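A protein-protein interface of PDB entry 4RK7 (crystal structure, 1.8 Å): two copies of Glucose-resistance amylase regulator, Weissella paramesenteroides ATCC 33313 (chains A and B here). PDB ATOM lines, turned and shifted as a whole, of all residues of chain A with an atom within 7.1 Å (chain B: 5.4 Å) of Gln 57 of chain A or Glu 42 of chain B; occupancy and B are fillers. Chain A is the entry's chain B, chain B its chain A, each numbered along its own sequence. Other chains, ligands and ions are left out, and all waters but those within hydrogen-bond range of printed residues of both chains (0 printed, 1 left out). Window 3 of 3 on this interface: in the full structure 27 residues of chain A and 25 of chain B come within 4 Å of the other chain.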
ATOM      1  N   THR A  46     -24.695 -18.951 -28.319  1.00  0.00           N
ATOM      2  CA  THR A  46     -25.044 -17.585 -28.018  1.00  0.00           C
ATOM      3  C   THR A  46     -25.717 -16.957 -29.239  1.00  0.00           C
ATOM      4  O   THR A  46     -25.449 -17.327 -30.390  1.00  0.00           O
ATOM      5  CB  THR A  46     -23.800 -16.785 -27.540  1.00  0.00           C
ATOM      6  OG1 THR A  46     -24.208 -15.505 -27.050  1.00  0.00           O
ATOM      7  CG2 THR A  46     -22.792 -16.601 -28.662  1.00  0.00           C
ATOM      8  N   TYR A  47     -26.632 -16.030 -28.988  1.00  0.00           N
ATOM      9  CA  TYR A  47     -27.342 -15.374 -30.073  1.00  0.00           C
ATOM     10  C   TYR A  47     -26.826 -13.933 -30.259  1.00  0.00           C
ATOM     11  O   TYR A  47     -26.342 -13.307 -29.313  1.00  0.00           O
ATOM     12  CB  TYR A  47     -28.866 -15.410 -29.850  1.00  0.00           C
ATOM     13  CG  TYR A  47     -29.465 -16.798 -30.002  1.00  0.00           C
ATOM     14  CD1 TYR A  47     -29.363 -17.745 -28.984  1.00  0.00           C
ATOM     15  CD2 TYR A  47     -30.115 -17.169 -31.174  1.00  0.00           C
ATOM     16  CE1 TYR A  47     -29.902 -19.015 -29.129  1.00  0.00           C
ATOM     17  CE2 TYR A  47     -30.656 -18.436 -31.329  1.00  0.00           C
ATOM     18  CZ  TYR A  47     -30.547 -19.355 -30.305  1.00  0.00           C
ATOM     19  OH  TYR A  47     -31.080 -20.616 -30.456  1.00  0.00           O
ATOM     20  N   ASP A  51     -27.439  -4.937 -32.542  1.00  0.00           N
ATOM     21  CA  ASP A  51     -27.031  -3.833 -31.692  1.00  0.00           C
ATOM     22  C   ASP A  51     -25.571  -4.021 -31.290  1.00  0.00           C
ATOM     23  O   ASP A  51     -25.220  -4.984 -30.622  1.00  0.00           O
ATOM     24  CB  ASP A  51     -27.920  -3.764 -30.447  1.00  0.00           C
ATOM     25  CG  ASP A  51     -27.554  -2.616 -29.523  1.00  0.00           C
ATOM     26  OD1 ASP A  51     -26.461  -2.652 -28.916  1.00  0.00           O
ATOM     27  OD2 ASP A  51     -28.375  -1.689 -29.381  1.00  0.00           O
ATOM     28  N   GLU A  52     -24.720  -3.079 -31.673  1.00  0.00           N
ATOM     29  CA  GLU A  52     -23.284  -3.253 -31.497  1.00  0.00           C
ATOM     30  C   GLU A  52     -22.835  -3.348 -30.050  1.00  0.00           C
ATOM     31  O   GLU A  52     -21.859  -4.034 -29.762  1.00  0.00           O
ATOM     32  CB  GLU A  52     -22.508  -2.137 -32.224  1.00  0.00           C
ATOM     33  CG  GLU A  52     -21.061  -2.503 -32.522  1.00  0.00           C
ATOM     34  CD  GLU A  52     -20.465  -1.671 -33.641  1.00  0.00           C
ATOM     35  OE1 GLU A  52     -19.932  -2.273 -34.614  1.00  0.00           O
ATOM     36  OE2 GLU A  52     -20.541  -0.423 -33.544  1.00  0.00           O
ATOM     37  N   ASP A  53     -23.538  -2.688 -29.132  1.00  0.00           N
ATOM     38  CA  ASP A  53     -23.197  -2.776 -27.700  1.00  0.00           C
ATOM     39  C   ASP A  53     -23.499  -4.157 -27.123  1.00  0.00           C
ATOM     40  O   ASP A  53     -22.786  -4.643 -26.247  1.00  0.00           O
ATOM     41  CB  ASP A  53     -23.966  -1.735 -26.885  1.00  0.00           C
ATOM     42  CG  ASP A  53     -23.554  -0.327 -27.217  1.00  0.00           C
ATOM     43  OD1 ASP A  53     -22.359  -0.008 -27.039  1.00  0.00           O
ATOM     44  OD2 ASP A  53     -24.425   0.454 -27.653  1.00  0.00           O
ATOM     45  N   HIS A  54     -24.573  -4.765 -27.604  1.00  0.00           N
ATOM     46  CA  HIS A  54     -24.944  -6.107 -27.164  1.00  0.00           C
ATOM     47  C   HIS A  54     -23.954  -7.098 -27.735  1.00  0.00           C
ATOM     48  O   HIS A  54     -23.531  -8.014 -27.043  1.00  0.00           O
ATOM     49  CB  HIS A  54     -26.361  -6.462 -27.608  1.00  0.00           C
ATOM     50  CG  HIS A  54     -27.417  -5.574 -27.020  1.00  0.00           C
ATOM     51  ND1 HIS A  54     -28.690  -5.481 -27.543  1.00  0.00           N
ATOM     52  CD2 HIS A  54     -27.380  -4.718 -25.970  1.00  0.00           C
ATOM     53  CE1 HIS A  54     -29.394  -4.614 -26.834  1.00  0.00           C
ATOM     54  NE2 HIS A  54     -28.621  -4.136 -25.875  1.00  0.00           N
ATOM     55  N   GLN A  55     -23.581  -6.901 -29.000  1.00  0.00           N
ATOM     56  CA  GLN A  55     -22.549  -7.727 -29.638  1.00  0.00           C
ATOM     57  C   GLN A  55     -21.265  -7.714 -28.815  1.00  0.00           C
ATOM     58  O   GLN A  55     -20.633  -8.754 -28.587  1.00  0.00           O
ATOM     59  CB  GLN A  55     -22.277  -7.231 -31.055  1.00  0.00           C
ATOM     60  CG  GLN A  55     -23.408  -7.510 -32.026  1.00  0.00           C
ATOM     61  CD  GLN A  55     -23.229  -6.816 -33.361  1.00  0.00           C
ATOM     62  OE1 GLN A  55     -22.303  -6.013 -33.544  1.00  0.00           O
ATOM     63  NE2 GLN A  55     -24.115  -7.115 -34.305  1.00  0.00           N
ATOM     64  N   TYR A  56     -20.863  -6.545 -28.349  1.00  0.00           N
ATOM     65  CA  TYR A  56     -19.635  -6.469 -27.561  1.00  0.00           C
ATOM     66  C   TYR A  56     -19.743  -7.200 -26.215  1.00  0.00           C
ATOM     67  O   TYR A  56     -18.786  -7.857 -25.794  1.00  0.00           O
ATOM     68  CB  TYR A  56     -19.229  -5.021 -27.343  1.00  0.00           C
ATOM     69  CG  TYR A  56     -17.882  -4.889 -26.691  1.00  0.00           C
ATOM     70  CD1 TYR A  56     -16.721  -5.190 -27.393  1.00  0.00           C
ATOM     71  CD2 TYR A  56     -17.764  -4.479 -25.370  1.00  0.00           C
ATOM     72  CE1 TYR A  56     -15.478  -5.082 -26.798  1.00  0.00           C
ATOM     73  CE2 TYR A  56     -16.524  -4.360 -24.766  1.00  0.00           C
ATOM     74  CZ  TYR A  56     -15.385  -4.666 -25.484  1.00  0.00           C
ATOM     75  OH  TYR A  56     -14.148  -4.553 -24.893  1.00  0.00           O
ATOM     76  N   GLN A  57     -20.893  -7.076 -25.545  1.00  0.00           N
ATOM     77  CA  GLN A  57     -21.118  -7.760 -24.262  1.00  0.00           C
ATOM     78  C   GLN A  57     -21.001  -9.266 -24.458  1.00  0.00           C
ATOM     79  O   GLN A  57     -20.317  -9.939 -23.692  1.00  0.00           O
ATOM     80  CB  GLN A  57     -22.491  -7.433 -23.650  1.00  0.00           C
ATOM     81  CG  GLN A  57     -22.806  -5.955 -23.428  1.00  0.00           C
ATOM     82  CD  GLN A  57     -21.599  -5.115 -23.027  1.00  0.00           C
ATOM     83  OE1 GLN A  57     -20.891  -5.436 -22.069  1.00  0.00           O
ATOM     84  NE2 GLN A  57     -21.369  -4.021 -23.753  1.00  0.00           N
ATOM     85  N   VAL A  58     -21.648  -9.769 -25.508  1.00  0.00           N
ATOM     86  CA  VAL A  58     -21.537 -11.166 -25.920  1.00  0.00           C
ATOM     87  C   VAL A  58     -20.101 -11.612 -26.143  1.00  0.00           C
ATOM     88  O   VAL A  58     -19.691 -12.670 -25.667  1.00  0.00           O
ATOM     89  CB  VAL A  58     -22.330 -11.422 -27.228  1.00  0.00           C
ATOM     90  CG1 VAL A  58     -21.924 -12.738 -27.886  1.00  0.00           C
ATOM     91  CG2 VAL A  58     -23.826 -11.402 -26.951  1.00  0.00           C
ATOM     92  N   PHE A  59     -19.339 -10.822 -26.890  1.00  0.00           N
ATOM     93  CA  PHE A  59     -17.946 -11.156 -27.130  1.00  0.00           C
ATOM     94  C   PHE A  59     -17.156 -11.338 -25.816  1.00  0.00           C
ATOM     95  O   PHE A  59     -16.395 -12.292 -25.653  1.00  0.00           O
ATOM     96  CB  PHE A  59     -17.289 -10.105 -28.023  1.00  0.00           C
ATOM     97  CG  PHE A  59     -15.811 -10.066 -27.880  1.00  0.00           C
ATOM     98  CD1 PHE A  59     -15.017 -11.000 -28.527  1.00  0.00           C
ATOM     99  CD2 PHE A  59     -15.207  -9.120 -27.071  1.00  0.00           C
ATOM    100  CE1 PHE A  59     -13.645 -10.982 -28.376  1.00  0.00           C
ATOM    101  CE2 PHE A  59     -13.835  -9.107 -26.914  1.00  0.00           C
ATOM    102  CZ  PHE A  59     -13.055 -10.047 -27.561  1.00  0.00           C
ATOM    103  N   GLN A  60     -17.336 -10.429 -24.868  1.00  0.00           N
ATOM    104  CA  GLN A  60     -16.767 -10.630 -23.532  1.00  0.00           C
ATOM    105  C   GLN A  60     -17.220 -11.960 -22.886  1.00  0.00           C
ATOM    106  O   GLN A  60     -16.453 -12.537 -22.128  1.00  0.00           O
ATOM    107  CB  GLN A  60     -17.084  -9.442 -22.630  1.00  0.00           C
ATOM    108  CG  GLN A  60     -16.460  -8.143 -23.127  1.00  0.00           C
ATOM    109  CD  GLN A  60     -16.896  -6.906 -22.357  1.00  0.00           C
ATOM    110  OE1 GLN A  60     -16.081  -6.029 -22.077  1.00  0.00           O
ATOM    111  NE2 GLN A  60     -18.182  -6.819 -22.027  1.00  0.00           N
ATOM    112  N   THR A  61     -18.435 -12.435 -23.209  1.00  0.00           N
ATOM    113  CA  THR A  61     -18.938 -13.793 -22.821  1.00  0.00           C
ATOM    114  C   THR A  61     -18.182 -14.941 -23.566  1.00  0.00           C
ATOM    115  O   THR A  61     -17.978 -16.005 -23.022  1.00  0.00           O
ATOM    116  CB  THR A  61     -20.482 -13.889 -22.997  1.00  0.00           C
ATOM    117  OG1 THR A  61     -21.122 -13.175 -21.932  1.00  0.00           O
ATOM    118  CG2 THR A  61     -20.999 -15.333 -22.999  1.00  0.00           C
ATOM    119  N   LEU A  62     -17.747 -14.721 -24.801  1.00  0.00           N
ATOM    120  CA  LEU A  62     -16.869 -15.679 -25.498  1.00  0.00           C
ATOM    121  C   LEU A  62     -15.430 -15.671 -24.999  1.00  0.00           C
ATOM    122  O   LEU A  62     -14.853 -16.729 -24.750  1.00  0.00           O
ATOM    123  CB  LEU A  62     -16.889 -15.401 -26.992  1.00  0.00           C
ATOM    124  CG  LEU A  62     -18.238 -15.661 -27.658  1.00  0.00           C
ATOM    125  CD1 LEU A  62     -18.220 -15.132 -29.082  1.00  0.00           C
ATOM    126  CD2 LEU A  62     -18.599 -17.136 -27.636  1.00  0.00           C
ATOM    127  N   SER A  64     -14.346 -14.549 -21.989  1.00  0.00           N
ATOM    128  CA  SER A  64     -14.312 -14.919 -20.561  1.00  0.00           C
ATOM    129  C   SER A  64     -14.750 -16.355 -20.272  1.00  0.00           C
ATOM    130  O   SER A  64     -14.620 -16.835 -19.151  1.00  0.00           O
ATOM    131  CB  SER A  64     -15.183 -13.964 -19.739  1.00  0.00           C
ATOM    132  OG  SER A  64     -16.551 -14.110 -20.077  1.00  0.00           O
ATOM    133  N   ARG A  65     -15.290 -17.031 -21.278  1.00  0.00           N
ATOM    134  CA  ARG A  65     -15.514 -18.465 -21.195  1.00  0.00           C
ATOM    135  C   ARG A  65     -14.279 -19.197 -21.747  1.00  0.00           C
ATOM    136  O   ARG A  65     -14.257 -20.426 -21.827  1.00  0.00           O
ATOM    137  CB  ARG A  65     -16.791 -18.847 -21.959  1.00  0.00           C
ATOM    138  CG  ARG A  65     -18.096 -18.646 -21.184  1.00  0.00           C
ATOM    139  CD  ARG A  65     -18.300 -17.258 -20.579  1.00  0.00           C
ATOM    140  NE  ARG A  65     -18.624 -17.288 -19.152  1.00  0.00           N
ATOM    141  CZ  ARG A  65     -18.869 -16.205 -18.412  1.00  0.00           C
ATOM    142  NH1 ARG A  65     -18.838 -14.989 -18.953  1.00  0.00           N
ATOM    143  NH2 ARG A  65     -19.149 -16.336 -17.117  1.00  0.00           N
ATOM    144  N   TRP A  80     -14.606  -6.331 -36.192  1.00  0.00           N
ATOM    145  CA  TRP A  80     -13.860  -6.195 -34.957  1.00  0.00           C
ATOM    146  C   TRP A  80     -14.014  -7.419 -34.072  1.00  0.00           C
ATOM    147  O   TRP A  80     -13.105  -7.720 -33.339  1.00  0.00           O
ATOM    148  CB  TRP A  80     -14.204  -4.925 -34.161  1.00  0.00           C
ATOM    149  CG  TRP A  80     -15.641  -4.753 -33.772  1.00  0.00           C
ATOM    150  CD1 TRP A  80     -16.540  -3.920 -34.355  1.00  0.00           C
ATOM    151  CD2 TRP A  80     -16.333  -5.408 -32.696  1.00  0.00           C
ATOM    152  NE1 TRP A  80     -17.753  -4.021 -33.724  1.00  0.00           N
ATOM    153  CE2 TRP A  80     -17.657  -4.932 -32.710  1.00  0.00           C
ATOM    154  CE3 TRP A  80     -15.964  -6.356 -31.729  1.00  0.00           C
ATOM    155  CZ2 TRP A  80     -18.628  -5.378 -31.793  1.00  0.00           C
ATOM    156  CZ3 TRP A  80     -16.924  -6.795 -30.818  1.00  0.00           C
ATOM    157  CH2 TRP A  80     -18.243  -6.301 -30.863  1.00  0.00           C
ATOM    158  N   MET A  81     -15.146  -8.113 -34.147  1.00  0.00           N
ATOM    159  CA  MET A  81     -15.323  -9.342 -33.364  1.00  0.00           C
ATOM    160  C   MET A  81     -14.428 -10.445 -33.861  1.00  0.00           C
ATOM    161  O   MET A  81     -13.797 -11.149 -33.064  1.00  0.00           O
ATOM    162  CB  MET A  81     -16.768  -9.883 -33.410  1.00  0.00           C
ATOM    163  CG  MET A  81     -16.900 -10.933 -32.296  1.00  0.00           C
ATOM    164  SD  MET A  81     -18.770 -11.559 -32.309  1.00  0.00           S
ATOM    165  CE  MET A  81     -19.590  -9.871 -31.773  1.00  0.00           C
ATOM    166  N   ARG B  11     -22.387 -11.978 -14.231  1.00  0.00           N
ATOM    167  CA  ARG B  11     -23.793 -11.781 -14.696  1.00  0.00           C
ATOM    168  C   ARG B  11     -24.113 -12.610 -15.947  1.00  0.00           C
ATOM    169  O   ARG B  11     -24.315 -12.087 -17.033  1.00  0.00           O
ATOM    170  CB  ARG B  11     -24.086 -10.291 -14.917  1.00  0.00           C
ATOM    171  CG  ARG B  11     -24.546  -9.591 -13.648  1.00  0.00           C
ATOM    172  CD  ARG B  11     -24.673  -8.083 -13.816  1.00  0.00           C
ATOM    173  NE  ARG B  11     -25.978  -7.577 -13.378  1.00  0.00           N
ATOM    174  CZ  ARG B  11     -26.450  -7.620 -12.128  1.00  0.00           C
ATOM    175  NH1 ARG B  11     -25.748  -8.168 -11.137  1.00  0.00           N
ATOM    176  NH2 ARG B  11     -27.654  -7.124 -11.866  1.00  0.00           N
ATOM    177  N   VAL B  12     -24.185 -13.928 -15.759  1.00  0.00           N
ATOM    178  CA  VAL B  12     -24.577 -14.851 -16.820  1.00  0.00           C
ATOM    179  C   VAL B  12     -25.679 -15.773 -16.291  1.00  0.00           C
ATOM    180  O   VAL B  12     -25.650 -16.141 -15.114  1.00  0.00           O
ATOM    181  CB  VAL B  12     -23.376 -15.691 -17.287  1.00  0.00           C
ATOM    182  CG1 VAL B  12     -23.801 -16.736 -18.307  1.00  0.00           C
ATOM    183  CG2 VAL B  12     -22.310 -14.781 -17.878  1.00  0.00           C
ATOM    184  N   VAL B  13     -26.656 -16.085 -17.140  1.00  0.00           N
ATOM    185  CA  VAL B  13     -27.658 -17.109 -16.831  1.00  0.00           C
ATOM    186  C   VAL B  13     -27.589 -18.174 -17.903  1.00  0.00           C
ATOM    187  O   VAL B  13     -27.280 -17.897 -19.055  1.00  0.00           O
ATOM    188  CB  VAL B  13     -29.098 -16.567 -16.717  1.00  0.00           C
ATOM    189  CG1 VAL B  13     -29.203 -15.593 -15.544  1.00  0.00           C
ATOM    190  CG2 VAL B  13     -29.568 -15.918 -18.001  1.00  0.00           C
ATOM    191  N   THR B  36     -32.954 -10.439 -20.103  1.00  0.00           N
ATOM    192  CA  THR B  36     -31.537 -10.501 -19.710  1.00  0.00           C
ATOM    193  C   THR B  36     -30.783  -9.283 -20.218  1.00  0.00           C
ATOM    194  O   THR B  36     -30.025  -8.652 -19.472  1.00  0.00           O
ATOM    195  CB  THR B  36     -30.794 -11.753 -20.240  1.00  0.00           C
ATOM    196  OG1 THR B  36     -30.807 -11.772 -21.676  1.00  0.00           O
ATOM    197  CG2 THR B  36     -31.407 -13.022 -19.690  1.00  0.00           C
ATOM    198  N   ILE B  37     -30.998  -8.960 -21.489  1.00  0.00           N
ATOM    199  CA  ILE B  37     -30.258  -7.879 -22.141  1.00  0.00           C
ATOM    200  C   ILE B  37     -30.489  -6.542 -21.419  1.00  0.00           C
ATOM    201  O   ILE B  37     -29.543  -5.797 -21.147  1.00  0.00           O
ATOM    202  CB  ILE B  37     -30.599  -7.800 -23.663  1.00  0.00           C
ATOM    203  CG1 ILE B  37     -29.318  -7.721 -24.500  1.00  0.00           C
ATOM    204  CG2 ILE B  37     -31.575  -6.667 -23.989  1.00  0.00           C
ATOM    205  CD1 ILE B  37     -28.550  -9.026 -24.560  1.00  0.00           C
ATOM    206  N   GLY B  40     -28.651  -6.336 -17.899  1.00  0.00           N
ATOM    207  CA  GLY B  40     -27.190  -6.456 -17.841  1.00  0.00           C
ATOM    208  C   GLY B  40     -26.638  -7.871 -17.686  1.00  0.00           C
ATOM    209  O   GLY B  40     -25.488  -8.054 -17.273  1.00  0.00           O
ATOM    210  N   TYR B  41     -27.451  -8.876 -18.009  1.00  0.00           N
ATOM    211  CA  TYR B  41     -27.015 -10.282 -17.982  1.00  0.00           C
ATOM    212  C   TYR B  41     -26.768 -10.749 -19.412  1.00  0.00           C
ATOM    213  O   TYR B  41     -27.283 -10.165 -20.372  1.00  0.00           O
ATOM    214  CB  TYR B  41     -28.095 -11.186 -17.356  1.00  0.00           C
ATOM    215  CG  TYR B  41     -28.034 -11.285 -15.846  1.00  0.00           C
ATOM    216  CD1 TYR B  41     -28.566 -10.289 -15.042  1.00  0.00           C
ATOM    217  CD2 TYR B  41     -27.431 -12.376 -15.236  1.00  0.00           C
ATOM    218  CE1 TYR B  41     -28.500 -10.380 -13.662  1.00  0.00           C
ATOM    219  CE2 TYR B  41     -27.365 -12.482 -13.864  1.00  0.00           C
ATOM    220  CZ  TYR B  41     -27.903 -11.476 -13.082  1.00  0.00           C
ATOM    221  OH  TYR B  41     -27.839 -11.572 -11.722  1.00  0.00           O
ATOM    222  N   GLU B  42     -25.991 -11.816 -19.540  1.00  0.00           N
ATOM    223  CA  GLU B  42     -25.849 -12.528 -20.803  1.00  0.00           C
ATOM    224  C   GLU B  42     -26.390 -13.949 -20.657  1.00  0.00           C
ATOM    225  O   GLU B  42     -26.462 -14.482 -19.554  1.00  0.00           O
ATOM    226  CB  GLU B  42     -24.391 -12.529 -21.275  1.00  0.00           C
ATOM    227  CG  GLU B  42     -23.824 -11.135 -21.584  1.00  0.00           C
ATOM    228  CD  GLU B  42     -24.758 -10.251 -22.410  1.00  0.00           C
ATOM    229  OE1 GLU B  42     -25.020  -9.098 -21.999  1.00  0.00           O
ATOM    230  OE2 GLU B  42     -25.239 -10.702 -23.469  1.00  0.00           O
ATOM    231  N   LEU B  43     -26.803 -14.512 -21.785  1.00  0.00           N
ATOM    232  CA  LEU B  43     -27.498 -15.790 -21.854  1.00  0.00           C
ATOM    233  C   LEU B  43     -26.580 -16.849 -22.467  1.00  0.00           C
ATOM    234  O   LEU B  43     -26.028 -16.660 -23.546  1.00  0.00           O
ATOM    235  CB  LEU B  43     -28.754 -15.595 -22.698  1.00  0.00           C
ATOM    236  CG  LEU B  43     -29.832 -16.655 -22.666  1.00  0.00           C
ATOM    237  CD1 LEU B  43     -30.301 -16.860 -21.237  1.00  0.00           C
ATOM    238  CD2 LEU B  43     -30.977 -16.215 -23.560  1.00  0.00           C
ATOM    239  N   LEU B  44     -26.375 -17.946 -21.753  1.00  0.00           N
ATOM    240  CA  LEU B  44     -25.595 -19.069 -22.261  1.00  0.00           C
ATOM    241  C   LEU B  44     -26.576 -20.199 -22.531  1.00  0.00           C
ATOM    242  O   LEU B  44     -27.329 -20.577 -21.649  1.00  0.00           O
ATOM    243  CB  LEU B  44     -24.572 -19.452 -21.207  1.00  0.00           C
ATOM    244  CG  LEU B  44     -23.425 -20.376 -21.568  1.00  0.00           C
ATOM    245  CD1 LEU B  44     -22.263 -20.070 -20.641  1.00  0.00           C
ATOM    246  CD2 LEU B  44     -23.836 -21.839 -21.478  1.00  0.00           C
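The backbone NH of His 54 of chain A is in hydrogen-bond range of the side-chain carboxylate of Asp 51 of chain A, at 3.1 Å.
The backbone carbonyl oxygen (O) of Glu 42 of chain B sits at hydrogen-bond distance from the backbone NH (N) of Val 13 of chain B, 2.9 Å away.
The side-chain amide nitrogen (NE2) of Gln 57 of chain A is in hydrogen-bond range of the backbone carbonyl oxygen (O) of Asp 53 of chain A.
The backbone carbonyl oxygen (O) of Arg 11 of chain B lies within hydrogen-bond range of the backbone NH (N) of Glu 42 of chain B, 3.0 Å away.
NE2 of Gln 60 of chain A lies within hydrogen-bond range of OE1 of Gln 57 of chain A (3.0 Å).
The side-chain hydroxyl (OG) of Ser 64 of chain A is in hydrogen-bond range of the guanidinium group (NH1) of Arg 65 of chain A (2.7 Å).
Among the printed residues, pairs that only touch across the chains: His 54 of chain A with Ile 37 of chain B, Gln 57 of chain A with Glu 42 of chain B, Val 58 of chain A with Glu 42 of chain B, Thr 61 of chain A with Glu 42 of chain B and Arg 65 of chain A with Val 12 of chain B.
Gln 57 of chain A touches just one residue of chain B: Glu 42 (3.4 Å).
Of the printed residues of chain B, Val 58 of chain A touches Glu 42.
Phe 59 of chain A touches none of the printed residues of chain B.
Of the printed residues of chain B, Arg 65 of chain A touches Val 12.
Of the printed residues of chain A, Val 12 of chain B touches Arg 65.
Of the printed residues of chain A, Ile 37 of chain B touches His 54.
Glu 42 of chain B touches just these residues of chain A: Gln 57 (3.4 Å), Val 58 (3.8 Å) and Thr 61 (3.4 Å).
The nearest printed residue of chain B that does not touch Arg 65 of chain A is Leu 44 of chain B (4.4 Å).
Printed residues of chain A that touch a printed residue of chain B: His 54, Gln 57, Val 58, Thr 61 and Arg 65.
Of the 10 printed residues of chain B, 3 touch a printed residue of chain A.
Among the printed residues, 5 pairs touch across the chains.
No position is printed for both chains.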
